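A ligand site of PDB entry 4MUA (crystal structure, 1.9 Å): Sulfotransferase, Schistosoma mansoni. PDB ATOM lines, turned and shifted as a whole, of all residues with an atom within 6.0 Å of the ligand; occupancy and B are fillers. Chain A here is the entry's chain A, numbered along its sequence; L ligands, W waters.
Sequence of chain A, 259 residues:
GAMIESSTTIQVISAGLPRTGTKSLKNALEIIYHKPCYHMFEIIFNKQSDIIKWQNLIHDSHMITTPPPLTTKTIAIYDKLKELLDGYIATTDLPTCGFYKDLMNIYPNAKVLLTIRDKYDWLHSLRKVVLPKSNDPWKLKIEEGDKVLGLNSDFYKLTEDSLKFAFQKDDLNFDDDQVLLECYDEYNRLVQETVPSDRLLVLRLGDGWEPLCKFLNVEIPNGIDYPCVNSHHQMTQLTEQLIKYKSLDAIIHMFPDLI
The side-chain hydroxyl (OG) of Ser 125 lies within hydrogen-bond range of the guanidinium group (NE) of Arg 19, at 2.7 Å. A ring nitrogen (NE2) of His 39 sits at hydrogen-bond distance from the side-chain hydroxyl of Thr 22 (2.8 Å). The guanidinium group (NH1) of Arg 117 sits at hydrogen-bond distance from the backbone carbonyl oxygen (O) of Arg 19 (2.8 Å). The backbone carbonyl oxygen (O) of Asn 230 sits at hydrogen-bond distance from the guanidinium group (NH2) of Arg 19 (3.0 Å). The side-chain hydroxyl (OG) of Ser 24 lies within hydrogen-bond range of the backbone carbonyl oxygen (O) of Pro 227 (3.1 Å). The side-chain hydroxyl (OG) of Ser 24 is in hydrogen-bond range of the backbone NH (N) of Val 229. The backbone NH of Lys 23 is in hydrogen-bond range of a ring nitrogen (NE2) of His 39. The backbone carbonyl oxygen of Leu 17 sits at hydrogen-bond distance from the side-chain hydroxyl of Thr 20 (2.7 Å).
Residues that only touch the ligand: Val 229, Ser 231, Leu 205, Cys 228, Gly 206, Tyr 226 and Pro 18. Hydrophobic or aromatic side chains within 4 Å of the ligand: Leu 205, Tyr 226 and His 232. The nearest printed residue that does not touch the ligand is His 39 (4.4 Å).
The side-chain hydroxyl of Ser 125 lies within hydrogen-bond range of an oxygen (O1) of the ligand, at 2.5 Å. An oxygen (O5) of the ligand lies within hydrogen-bond range of the backbone NH (N) of Thr 22, at 2.7 Å. The side-chain hydroxyl (OG1) of Thr 22 lies within hydrogen-bond range of an oxygen (O5) of the ligand (2.6 Å). An oxygen (O2) of the ligand lies within salt-bridge range of the guanidinium group (NH2) of Arg 117, 2.8 Å away. ND2 of Asn 230 sits at hydrogen-bond distance from O4 of the ligand (2.8 Å). The backbone NH (N) of Arg 19 lies within hydrogen-bond range of an oxygen (O5) of the ligand. O1 of the ligand lies within salt-bridge range of NH2 of Arg 19 (2.9 Å). O7 of the ligand is in hydrogen-bond range of N of Gly 21, 2.9 Å away. OG of Ser 24 is in hydrogen-bond range of N2 of the ligand (2.9 Å). N of Lys 23 lies within hydrogen-bond range of O4 of the ligand (2.9 Å). An oxygen (O1) of the ligand lies within hydrogen-bond range of the backbone NH (N) of His 232 (3.0 Å). N3 of the ligand is in hydrogen-bond range of O of Pro 227, at 3.1 Å. The backbone NH (N) of Thr 20 sits at hydrogen-bond distance from an oxygen (O5) of the ligand (3.4 Å).
Water W4 lies within hydrogen-bond range of O2 of the ligand (2.8 Å), O of Asp 121 (2.8 Å) and ND1 of His 124 (3.3 Å). Water W5 bridges O6 of the ligand and ND2 of Asn 230. Water W3 lies within hydrogen-bond range of the backbone NH (N) of Ser 24 (2.8 Å), an oxygen (O4) of the ligand (2.9 Å), the backbone carbonyl oxygen (O) of Val 229 (3.0 Å) and the backbone NH (N) of Lys 23 (3.4 Å). Water W1 bridges O10 of the ligand (3.0 Å) and SG of Cys 228 (3.4 Å). Water W2 lies within hydrogen-bond range of N of Gly 206 (3.1 Å) and N3 of the ligand (3.4 Å).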
ATOM      1  N   LEU A  17      -8.077  13.174 -31.621  1.00  0.00           N
ATOM      2  CA  LEU A  17      -7.921  12.532 -30.304  1.00  0.00           C
ATOM      3  C   LEU A  17      -9.096  11.641 -29.975  1.00  0.00           C
ATOM      4  O   LEU A  17     -10.152  11.775 -30.576  1.00  0.00           O
ATOM      5  CB  LEU A  17      -7.777  13.615 -29.235  1.00  0.00           C
ATOM      6  CG  LEU A  17      -6.477  14.419 -29.339  1.00  0.00           C
ATOM      7  CD1 LEU A  17      -6.492  15.605 -28.390  1.00  0.00           C
ATOM      8  CD2 LEU A  17      -5.294  13.539 -29.070  1.00  0.00           C
ATOM      9  N   PRO A  18      -8.931  10.712 -29.016  1.00  0.00           N
ATOM     10  CA  PRO A  18     -10.096   9.913 -28.634  1.00  0.00           C
ATOM     11  C   PRO A  18     -11.236  10.803 -28.156  1.00  0.00           C
ATOM     12  O   PRO A  18     -10.970  11.863 -27.611  1.00  0.00           O
ATOM     13  CB  PRO A  18      -9.566   9.067 -27.455  1.00  0.00           C
ATOM     14  CG  PRO A  18      -8.311   9.738 -27.027  1.00  0.00           C
ATOM     15  CD  PRO A  18      -7.728  10.303 -28.269  1.00  0.00           C
ATOM     16  N   ARG A  19     -12.468  10.356 -28.379  1.00  0.00           N
ATOM     17  CA  ARG A  19     -13.695  11.057 -27.990  1.00  0.00           C
ATOM     18  C   ARG A  19     -14.024  12.260 -28.876  1.00  0.00           C
ATOM     19  O   ARG A  19     -14.729  13.171 -28.445  1.00  0.00           O
ATOM     20  CB  ARG A  19     -13.721  11.445 -26.494  1.00  0.00           C
ATOM     21  CG  ARG A  19     -13.343  10.308 -25.531  1.00  0.00           C
ATOM     22  CD  ARG A  19     -14.158   9.041 -25.817  1.00  0.00           C
ATOM     23  NE  ARG A  19     -15.586   9.230 -25.549  1.00  0.00           N
ATOM     24  CZ  ARG A  19     -16.523   8.329 -25.848  1.00  0.00           C
ATOM     25  NH1 ARG A  19     -16.187   7.183 -26.436  1.00  0.00           N
ATOM     26  NH2 ARG A  19     -17.789   8.568 -25.557  1.00  0.00           N
ATOM     27  N   THR A  20     -13.524  12.249 -30.101  1.00  0.00           N
ATOM     28  CA  THR A  20     -13.866  13.283 -31.079  1.00  0.00           C
ATOM     29  C   THR A  20     -14.554  12.680 -32.294  1.00  0.00           C
ATOM     30  O   THR A  20     -14.572  13.270 -33.368  1.00  0.00           O
ATOM     31  CB  THR A  20     -12.618  14.077 -31.515  1.00  0.00           C
ATOM     32  OG1 THR A  20     -11.718  13.207 -32.223  1.00  0.00           O
ATOM     33  CG2 THR A  20     -11.907  14.690 -30.301  1.00  0.00           C
ATOM     34  N   GLY A  21     -15.146  11.499 -32.135  1.00  0.00           N
ATOM     35  CA  GLY A  21     -15.853  10.833 -33.211  1.00  0.00           C
ATOM     36  C   GLY A  21     -15.023   9.846 -34.028  1.00  0.00           C
ATOM     37  O   GLY A  21     -15.346   9.551 -35.169  1.00  0.00           O
ATOM     38  N   THR A  22     -13.949   9.330 -33.434  1.00  0.00           N
ATOM     39  CA  THR A  22     -13.060   8.401 -34.140  1.00  0.00           C
ATOM     40  C   THR A  22     -13.715   7.074 -34.529  1.00  0.00           C
ATOM     41  O   THR A  22     -13.426   6.521 -35.591  1.00  0.00           O
ATOM     42  CB  THR A  22     -11.786   8.111 -33.326  1.00  0.00           C
ATOM     43  OG1 THR A  22     -12.124   7.343 -32.163  1.00  0.00           O
ATOM     44  CG2 THR A  22     -11.141   9.414 -32.887  1.00  0.00           C
ATOM     45  N   LYS A  23     -14.588   6.544 -33.664  1.00  0.00           N
ATOM     46  CA  LYS A  23     -15.219   5.266 -33.988  1.00  0.00           C
ATOM     47  C   LYS A  23     -16.250   5.411 -35.104  1.00  0.00           C
ATOM     48  O   LYS A  23     -16.401   4.512 -35.939  1.00  0.00           O
ATOM     49  CB  LYS A  23     -15.816   4.594 -32.747  1.00  0.00           C
ATOM     50  CG  LYS A  23     -16.481   3.234 -33.025  1.00  0.00           C
ATOM     51  CD  LYS A  23     -15.494   2.254 -33.621  1.00  0.00           C
ATOM     52  CE  LYS A  23     -15.913   0.777 -33.490  1.00  0.00           C
ATOM     53  NZ  LYS A  23     -17.098   0.381 -34.313  1.00  0.00           N
ATOM     54  N   SER A  24     -16.973   6.532 -35.139  1.00  0.00           N
ATOM     55  CA  SER A  24     -17.851   6.811 -36.263  1.00  0.00           C
ATOM     56  C   SER A  24     -17.062   6.991 -37.547  1.00  0.00           C
ATOM     57  O   SER A  24     -17.463   6.530 -38.610  1.00  0.00           O
ATOM     58  CB  SER A  24     -18.702   8.054 -35.995  1.00  0.00           C
ATOM     59  OG  SER A  24     -19.714   7.749 -35.051  1.00  0.00           O
ATOM     60  N   HIS A  39      -8.222   1.411 -35.047  1.00  0.00           N
ATOM     61  CA  HIS A  39      -8.913   2.105 -33.980  1.00  0.00           C
ATOM     62  C   HIS A  39      -8.579   1.318 -32.722  1.00  0.00           C
ATOM     63  O   HIS A  39      -8.187   0.164 -32.827  1.00  0.00           O
ATOM     64  CB  HIS A  39     -10.423   2.059 -34.198  1.00  0.00           C
ATOM     65  CG  HIS A  39     -11.215   2.918 -33.256  1.00  0.00           C
ATOM     66  ND1 HIS A  39     -11.726   2.461 -32.065  1.00  0.00           N
ATOM     67  CD2 HIS A  39     -11.607   4.214 -33.356  1.00  0.00           C
ATOM     68  CE1 HIS A  39     -12.388   3.435 -31.462  1.00  0.00           C
ATOM     69  NE2 HIS A  39     -12.328   4.513 -32.229  1.00  0.00           N
ATOM     70  N   ASP A  93      -7.807   7.224 -33.829  1.00  0.00           N
ATOM     71  CA  ASP A  93      -7.821   6.940 -32.404  1.00  0.00           C
ATOM     72  C   ASP A  93      -6.429   6.681 -31.822  1.00  0.00           C
ATOM     73  O   ASP A  93      -5.417   6.588 -32.545  1.00  0.00           O
ATOM     74  CB  ASP A  93      -8.759   5.746 -32.154  1.00  0.00           C
ATOM     75  CG  ASP A  93      -9.167   5.589 -30.700  1.00  0.00           C
ATOM     76  OD1 ASP A  93      -8.885   6.508 -29.911  1.00  0.00           O
ATOM     77  OD2 ASP A  93      -9.784   4.564 -30.369  1.00  0.00           O
ATOM     78  N   ARG A 117     -13.835  19.118 -31.595  1.00  0.00           N
ATOM     79  CA  ARG A 117     -15.116  19.374 -30.955  1.00  0.00           C
ATOM     80  C   ARG A 117     -14.887  20.291 -29.757  1.00  0.00           C
ATOM     81  O   ARG A 117     -13.756  20.524 -29.351  1.00  0.00           O
ATOM     82  CB  ARG A 117     -15.771  18.058 -30.507  1.00  0.00           C
ATOM     83  CG  ARG A 117     -15.187  17.499 -29.213  1.00  0.00           C
ATOM     84  CD  ARG A 117     -15.758  16.136 -28.854  1.00  0.00           C
ATOM     85  NE  ARG A 117     -17.159  16.203 -28.454  1.00  0.00           N
ATOM     86  CZ  ARG A 117     -17.809  15.216 -27.833  1.00  0.00           C
ATOM     87  NH1 ARG A 117     -17.171  14.093 -27.499  1.00  0.00           N
ATOM     88  NH2 ARG A 117     -19.081  15.368 -27.507  1.00  0.00           N
ATOM     89  N   ASP A 121     -16.945  19.490 -23.795  1.00  0.00           N
ATOM     90  CA  ASP A 121     -17.660  18.294 -24.232  1.00  0.00           C
ATOM     91  C   ASP A 121     -16.691  17.121 -24.331  1.00  0.00           C
ATOM     92  O   ASP A 121     -16.994  16.001 -23.908  1.00  0.00           O
ATOM     93  CB  ASP A 121     -18.309  18.480 -25.595  1.00  0.00           C
ATOM     94  CG  ASP A 121     -19.585  19.314 -25.538  1.00  0.00           C
ATOM     95  OD1 ASP A 121     -20.066  19.600 -24.417  1.00  0.00           O
ATOM     96  OD2 ASP A 121     -20.103  19.667 -26.627  1.00  0.00           O
ATOM     97  N   HIS A 124     -15.471  16.021 -20.747  1.00  0.00           N
ATOM     98  CA  HIS A 124     -16.590  15.297 -20.128  1.00  0.00           C
ATOM     99  C   HIS A 124     -16.720  13.873 -20.655  1.00  0.00           C
ATOM    100  O   HIS A 124     -16.851  12.915 -19.886  1.00  0.00           O
ATOM    101  CB  HIS A 124     -17.887  16.067 -20.394  1.00  0.00           C
ATOM    102  CG  HIS A 124     -19.089  15.469 -19.724  1.00  0.00           C
ATOM    103  ND1 HIS A 124     -20.177  15.007 -20.429  1.00  0.00           N
ATOM    104  CD2 HIS A 124     -19.383  15.291 -18.421  1.00  0.00           C
ATOM    105  CE1 HIS A 124     -21.086  14.551 -19.584  1.00  0.00           C
ATOM    106  NE2 HIS A 124     -20.632  14.714 -18.358  1.00  0.00           N
ATOM    107  N   SER A 125     -16.693  13.729 -21.985  1.00  0.00           N
ATOM    108  CA  SER A 125     -16.750  12.421 -22.626  1.00  0.00           C
ATOM    109  C   SER A 125     -15.536  11.561 -22.226  1.00  0.00           C
ATOM    110  O   SER A 125     -15.662  10.388 -21.856  1.00  0.00           O
ATOM    111  CB  SER A 125     -16.817  12.608 -24.153  1.00  0.00           C
ATOM    112  OG  SER A 125     -17.005  11.388 -24.829  1.00  0.00           O
ATOM    113  N   VAL A 129     -15.205   7.700 -20.071  1.00  0.00           N
ATOM    114  CA  VAL A 129     -14.856   6.504 -20.839  1.00  0.00           C
ATOM    115  C   VAL A 129     -13.374   6.099 -20.811  1.00  0.00           C
ATOM    116  O   VAL A 129     -13.047   4.949 -20.534  1.00  0.00           O
ATOM    117  CB  VAL A 129     -15.255   6.667 -22.313  1.00  0.00           C
ATOM    118  CG1 VAL A 129     -14.825   5.451 -23.127  1.00  0.00           C
ATOM    119  CG2 VAL A 129     -16.752   6.939 -22.451  1.00  0.00           C
ATOM    120  N   VAL A 130     -12.506   7.054 -21.126  1.00  0.00           N
ATOM    121  CA  VAL A 130     -11.107   6.784 -21.400  1.00  0.00           C
ATOM    122  C   VAL A 130     -10.233   7.042 -20.179  1.00  0.00           C
ATOM    123  O   VAL A 130      -9.288   6.303 -19.895  1.00  0.00           O
ATOM    124  CB  VAL A 130     -10.609   7.666 -22.569  1.00  0.00           C
ATOM    125  CG1 VAL A 130      -9.127   7.530 -22.771  1.00  0.00           C
ATOM    126  CG2 VAL A 130     -11.369   7.349 -23.836  1.00  0.00           C
ATOM    127  N   LEU A 205     -17.950  17.330 -35.317  1.00  0.00           N
ATOM    128  CA  LEU A 205     -19.037  16.387 -35.108  1.00  0.00           C
ATOM    129  C   LEU A 205     -20.314  16.893 -35.781  1.00  0.00           C
ATOM    130  O   LEU A 205     -20.650  18.068 -35.706  1.00  0.00           O
ATOM    131  CB  LEU A 205     -19.242  16.119 -33.605  1.00  0.00           C
ATOM    132  CG  LEU A 205     -18.118  15.342 -32.912  1.00  0.00           C
ATOM    133  CD1 LEU A 205     -18.321  15.265 -31.396  1.00  0.00           C
ATOM    134  CD2 LEU A 205     -17.993  13.935 -33.491  1.00  0.00           C
ATOM    135  N   GLY A 206     -21.027  16.010 -36.465  1.00  0.00           N
ATOM    136  CA  GLY A 206     -22.221  16.412 -37.176  1.00  0.00           C
ATOM    137  C   GLY A 206     -22.010  16.757 -38.651  1.00  0.00           C
ATOM    138  O   GLY A 206     -22.980  16.854 -39.403  1.00  0.00           O
ATOM    139  N   TYR A 226     -24.479   8.660 -42.058  1.00  0.00           N
ATOM    140  CA  TYR A 226     -23.146   8.759 -41.497  1.00  0.00           C
ATOM    141  C   TYR A 226     -23.207   8.187 -40.087  1.00  0.00           C
ATOM    142  O   TYR A 226     -24.137   8.485 -39.341  1.00  0.00           O
ATOM    143  CB  TYR A 226     -22.665  10.216 -41.488  1.00  0.00           C
ATOM    144  CG  TYR A 226     -21.237  10.332 -40.997  1.00  0.00           C
ATOM    145  CD1 TYR A 226     -20.168  10.214 -41.881  1.00  0.00           C
ATOM    146  CD2 TYR A 226     -20.968  10.531 -39.657  1.00  0.00           C
ATOM    147  CE1 TYR A 226     -18.863  10.299 -41.440  1.00  0.00           C
ATOM    148  CE2 TYR A 226     -19.677  10.622 -39.199  1.00  0.00           C
ATOM    149  CZ  TYR A 226     -18.629  10.509 -40.091  1.00  0.00           C
ATOM    150  OH  TYR A 226     -17.344  10.584 -39.615  1.00  0.00           O
ATOM    151  N   PRO A 227     -22.237   7.334 -39.726  1.00  0.00           N
ATOM    152  CA  PRO A 227     -22.284   6.667 -38.413  1.00  0.00           C
ATOM    153  C   PRO A 227     -22.337   7.637 -37.224  1.00  0.00           C
ATOM    154  O   PRO A 227     -21.703   8.704 -37.234  1.00  0.00           O
ATOM    155  CB  PRO A 227     -20.990   5.868 -38.386  1.00  0.00           C
ATOM    156  CG  PRO A 227     -20.716   5.579 -39.813  1.00  0.00           C
ATOM    157  CD  PRO A 227     -21.158   6.797 -40.570  1.00  0.00           C
ATOM    158  N   CYS A 228     -23.123   7.287 -36.206  1.00  0.00           N
ATOM    159  CA  CYS A 228     -23.179   8.042 -34.967  1.00  0.00           C
ATOM    160  C   CYS A 228     -23.202   7.054 -33.805  1.00  0.00           C
ATOM    161  O   CYS A 228     -24.263   6.702 -33.312  1.00  0.00           O
ATOM    162  CB  CYS A 228     -24.419   8.936 -34.935  1.00  0.00           C
ATOM    163  SG  CYS A 228     -24.513   9.965 -33.457  1.00  0.00           S
ATOM    164  N   VAL A 229     -22.014   6.597 -33.400  1.00  0.00           N
ATOM    165  CA  VAL A 229     -21.875   5.544 -32.405  1.00  0.00           C
ATOM    166  C   VAL A 229     -20.859   5.947 -31.345  1.00  0.00           C
ATOM    167  O   VAL A 229     -20.192   6.978 -31.474  1.00  0.00           O
ATOM    168  CB  VAL A 229     -21.414   4.212 -33.043  1.00  0.00           C
ATOM    169  CG1 VAL A 229     -22.418   3.738 -34.081  1.00  0.00           C
ATOM    170  CG2 VAL A 229     -20.035   4.356 -33.684  1.00  0.00           C
ATOM    171  N   ASN A 230     -20.743   5.132 -30.301  1.00  0.00           N
ATOM    172  CA  ASN A 230     -19.718   5.302 -29.275  1.00  0.00           C
ATOM    173  C   ASN A 230     -19.916   6.515 -28.372  1.00  0.00           C
ATOM    174  O   ASN A 230     -18.929   7.067 -27.872  1.00  0.00           O
ATOM    175  CB  ASN A 230     -18.313   5.299 -29.894  1.00  0.00           C
ATOM    176  CG  ASN A 230     -17.230   4.844 -28.907  1.00  0.00           C
ATOM    177  OD1 ASN A 230     -17.526   4.185 -27.914  1.00  0.00           O
ATOM    178  ND2 ASN A 230     -15.975   5.208 -29.196  1.00  0.00           N
ATOM    179  N   SER A 231     -21.168   6.928 -28.150  1.00  0.00           N
ATOM    180  CA  SER A 231     -21.470   7.973 -27.180  1.00  0.00           C
ATOM    181  C   SER A 231     -21.130   7.453 -25.795  1.00  0.00           C
ATOM    182  O   SER A 231     -21.128   6.246 -25.571  1.00  0.00           O
ATOM    183  CB  SER A 231     -22.956   8.343 -27.211  1.00  0.00           C
ATOM    184  OG  SER A 231     -23.755   7.255 -26.751  1.00  0.00           O
ATOM    185  N   HIS A 232     -20.827   8.341 -24.860  1.00  0.00           N
ATOM    186  CA  HIS A 232     -20.493   7.872 -23.528  1.00  0.00           C
ATOM    187  C   HIS A 232     -21.674   7.093 -22.915  1.00  0.00           C
ATOM    188  O   HIS A 232     -21.460   6.126 -22.208  1.00  0.00           O
ATOM    189  CB  HIS A 232     -19.969   8.994 -22.622  1.00  0.00           C
ATOM    190  CG  HIS A 232     -21.009   9.988 -22.206  1.00  0.00           C
ATOM    191  ND1 HIS A 232     -21.945   9.719 -21.231  1.00  0.00           N
ATOM    192  CD2 HIS A 232     -21.245  11.250 -22.624  1.00  0.00           C
ATOM    193  CE1 HIS A 232     -22.719  10.780 -21.063  1.00  0.00           C
ATOM    194  NE2 HIS A 232     -22.317  11.721 -21.900  1.00  0.00           N
ATOM    195  N   HIS A 233     -22.904   7.515 -23.242  1.00  0.00           N
ATOM    196  CA  HIS A 233     -24.089   6.798 -22.787  1.00  0.00           C
ATOM    197  C   HIS A 233     -24.050   5.345 -23.273  1.00  0.00           C
ATOM    198  O   HIS A 233     -24.418   4.431 -22.550  1.00  0.00           O
ATOM    199  CB  HIS A 233     -25.360   7.478 -23.296  1.00  0.00           C
ATOM    200  CG  HIS A 233     -25.617   8.822 -22.698  1.00  0.00           C
ATOM    201  ND1 HIS A 233     -25.936   9.010 -21.370  1.00  0.00           N
ATOM    202  CD2 HIS A 233     -25.635  10.058 -23.258  1.00  0.00           C
ATOM    203  CE1 HIS A 233     -26.122  10.286 -21.134  1.00  0.00           C
ATOM    204  NE2 HIS A 233     -25.940  10.954 -22.267  1.00  0.00           N
HETATM  205  P1  LIG L   1     -20.075  11.891 -26.351  1.00  0.00           P
HETATM  206  O1  LIG L   1     -19.434  10.892 -25.386  1.00  0.00           O
HETATM  207  O2  LIG L   1     -19.933  13.303 -25.852  1.00  0.00           O
HETATM  208  O3  LIG L   1     -21.515  11.516 -26.541  1.00  0.00           O
HETATM  209  P2  LIG L   1     -14.831   8.423 -30.139  1.00  0.00           P
HETATM  210  O4  LIG L   1     -15.428   7.348 -30.985  1.00  0.00           O
HETATM  211  O5  LIG L   1     -13.563   8.940 -30.768  1.00  0.00           O
HETATM  212  O6  LIG L   1     -14.609   7.870 -28.738  1.00  0.00           O
HETATM  213  O7  LIG L   1     -15.862   9.647 -30.049  1.00  0.00           O
HETATM  214  C1  LIG L   1     -17.132   9.442 -29.402  1.00  0.00           C
HETATM  215  C2  LIG L   1     -17.855  10.749 -29.220  1.00  0.00           C
HETATM  216  O8  LIG L   1     -18.206  11.322 -30.509  1.00  0.00           O
HETATM  217  C3  LIG L   1     -19.152  10.623 -28.481  1.00  0.00           C
HETATM  218  O9  LIG L   1     -19.335  11.857 -27.775  1.00  0.00           O
HETATM  219  C4  LIG L   1     -20.164  10.512 -29.553  1.00  0.00           C
HETATM  220  O10 LIG L   1     -21.464  10.892 -29.105  1.00  0.00           O
HETATM  221  C5  LIG L   1     -19.632  11.477 -30.553  1.00  0.00           C
HETATM  222  N1  LIG L   1     -20.066  11.241 -31.872  1.00  0.00           N
HETATM  223  C6  LIG L   1     -19.699  10.225 -32.665  1.00  0.00           C
HETATM  224  N2  LIG L   1     -20.298  10.326 -33.865  1.00  0.00           N
HETATM  225  C7  LIG L   1     -21.054  11.463 -33.836  1.00  0.00           C
HETATM  226  C8  LIG L   1     -21.905  12.116 -34.776  1.00  0.00           C
HETATM  227  N3  LIG L   1     -22.100  11.589 -36.065  1.00  0.00           N
HETATM  228  N4  LIG L   1     -22.518  13.257 -34.412  1.00  0.00           N
HETATM  229  C9  LIG L   1     -22.354  13.770 -33.201  1.00  0.00           C
HETATM  230  N5  LIG L   1     -21.583  13.203 -32.287  1.00  0.00           N
HETATM  231  C10 LIG L   1     -20.912  12.051 -32.564  1.00  0.00           C
HETATM  232  O   HOH W   1     -24.244  10.560 -30.086  1.00  0.00           O
HETATM  233  O   HOH W   2     -19.411  13.424 -37.018  1.00  0.00           O
HETATM  234  O   HOH W   3     -17.631   7.796 -32.767  1.00  0.00           O
HETATM  235  O   HOH W   4     -19.638  15.022 -23.697  1.00  0.00           O
HETATM  236  O   HOH W   5     -13.139   5.751 -27.719  1.00  0.00           O
HETATM  237  O   HOH W   6     -24.066  11.640 -25.603  1.00  0.00           O
HETATM  238  O   HOH W   7     -24.556  14.767 -35.334  1.00  0.00           O
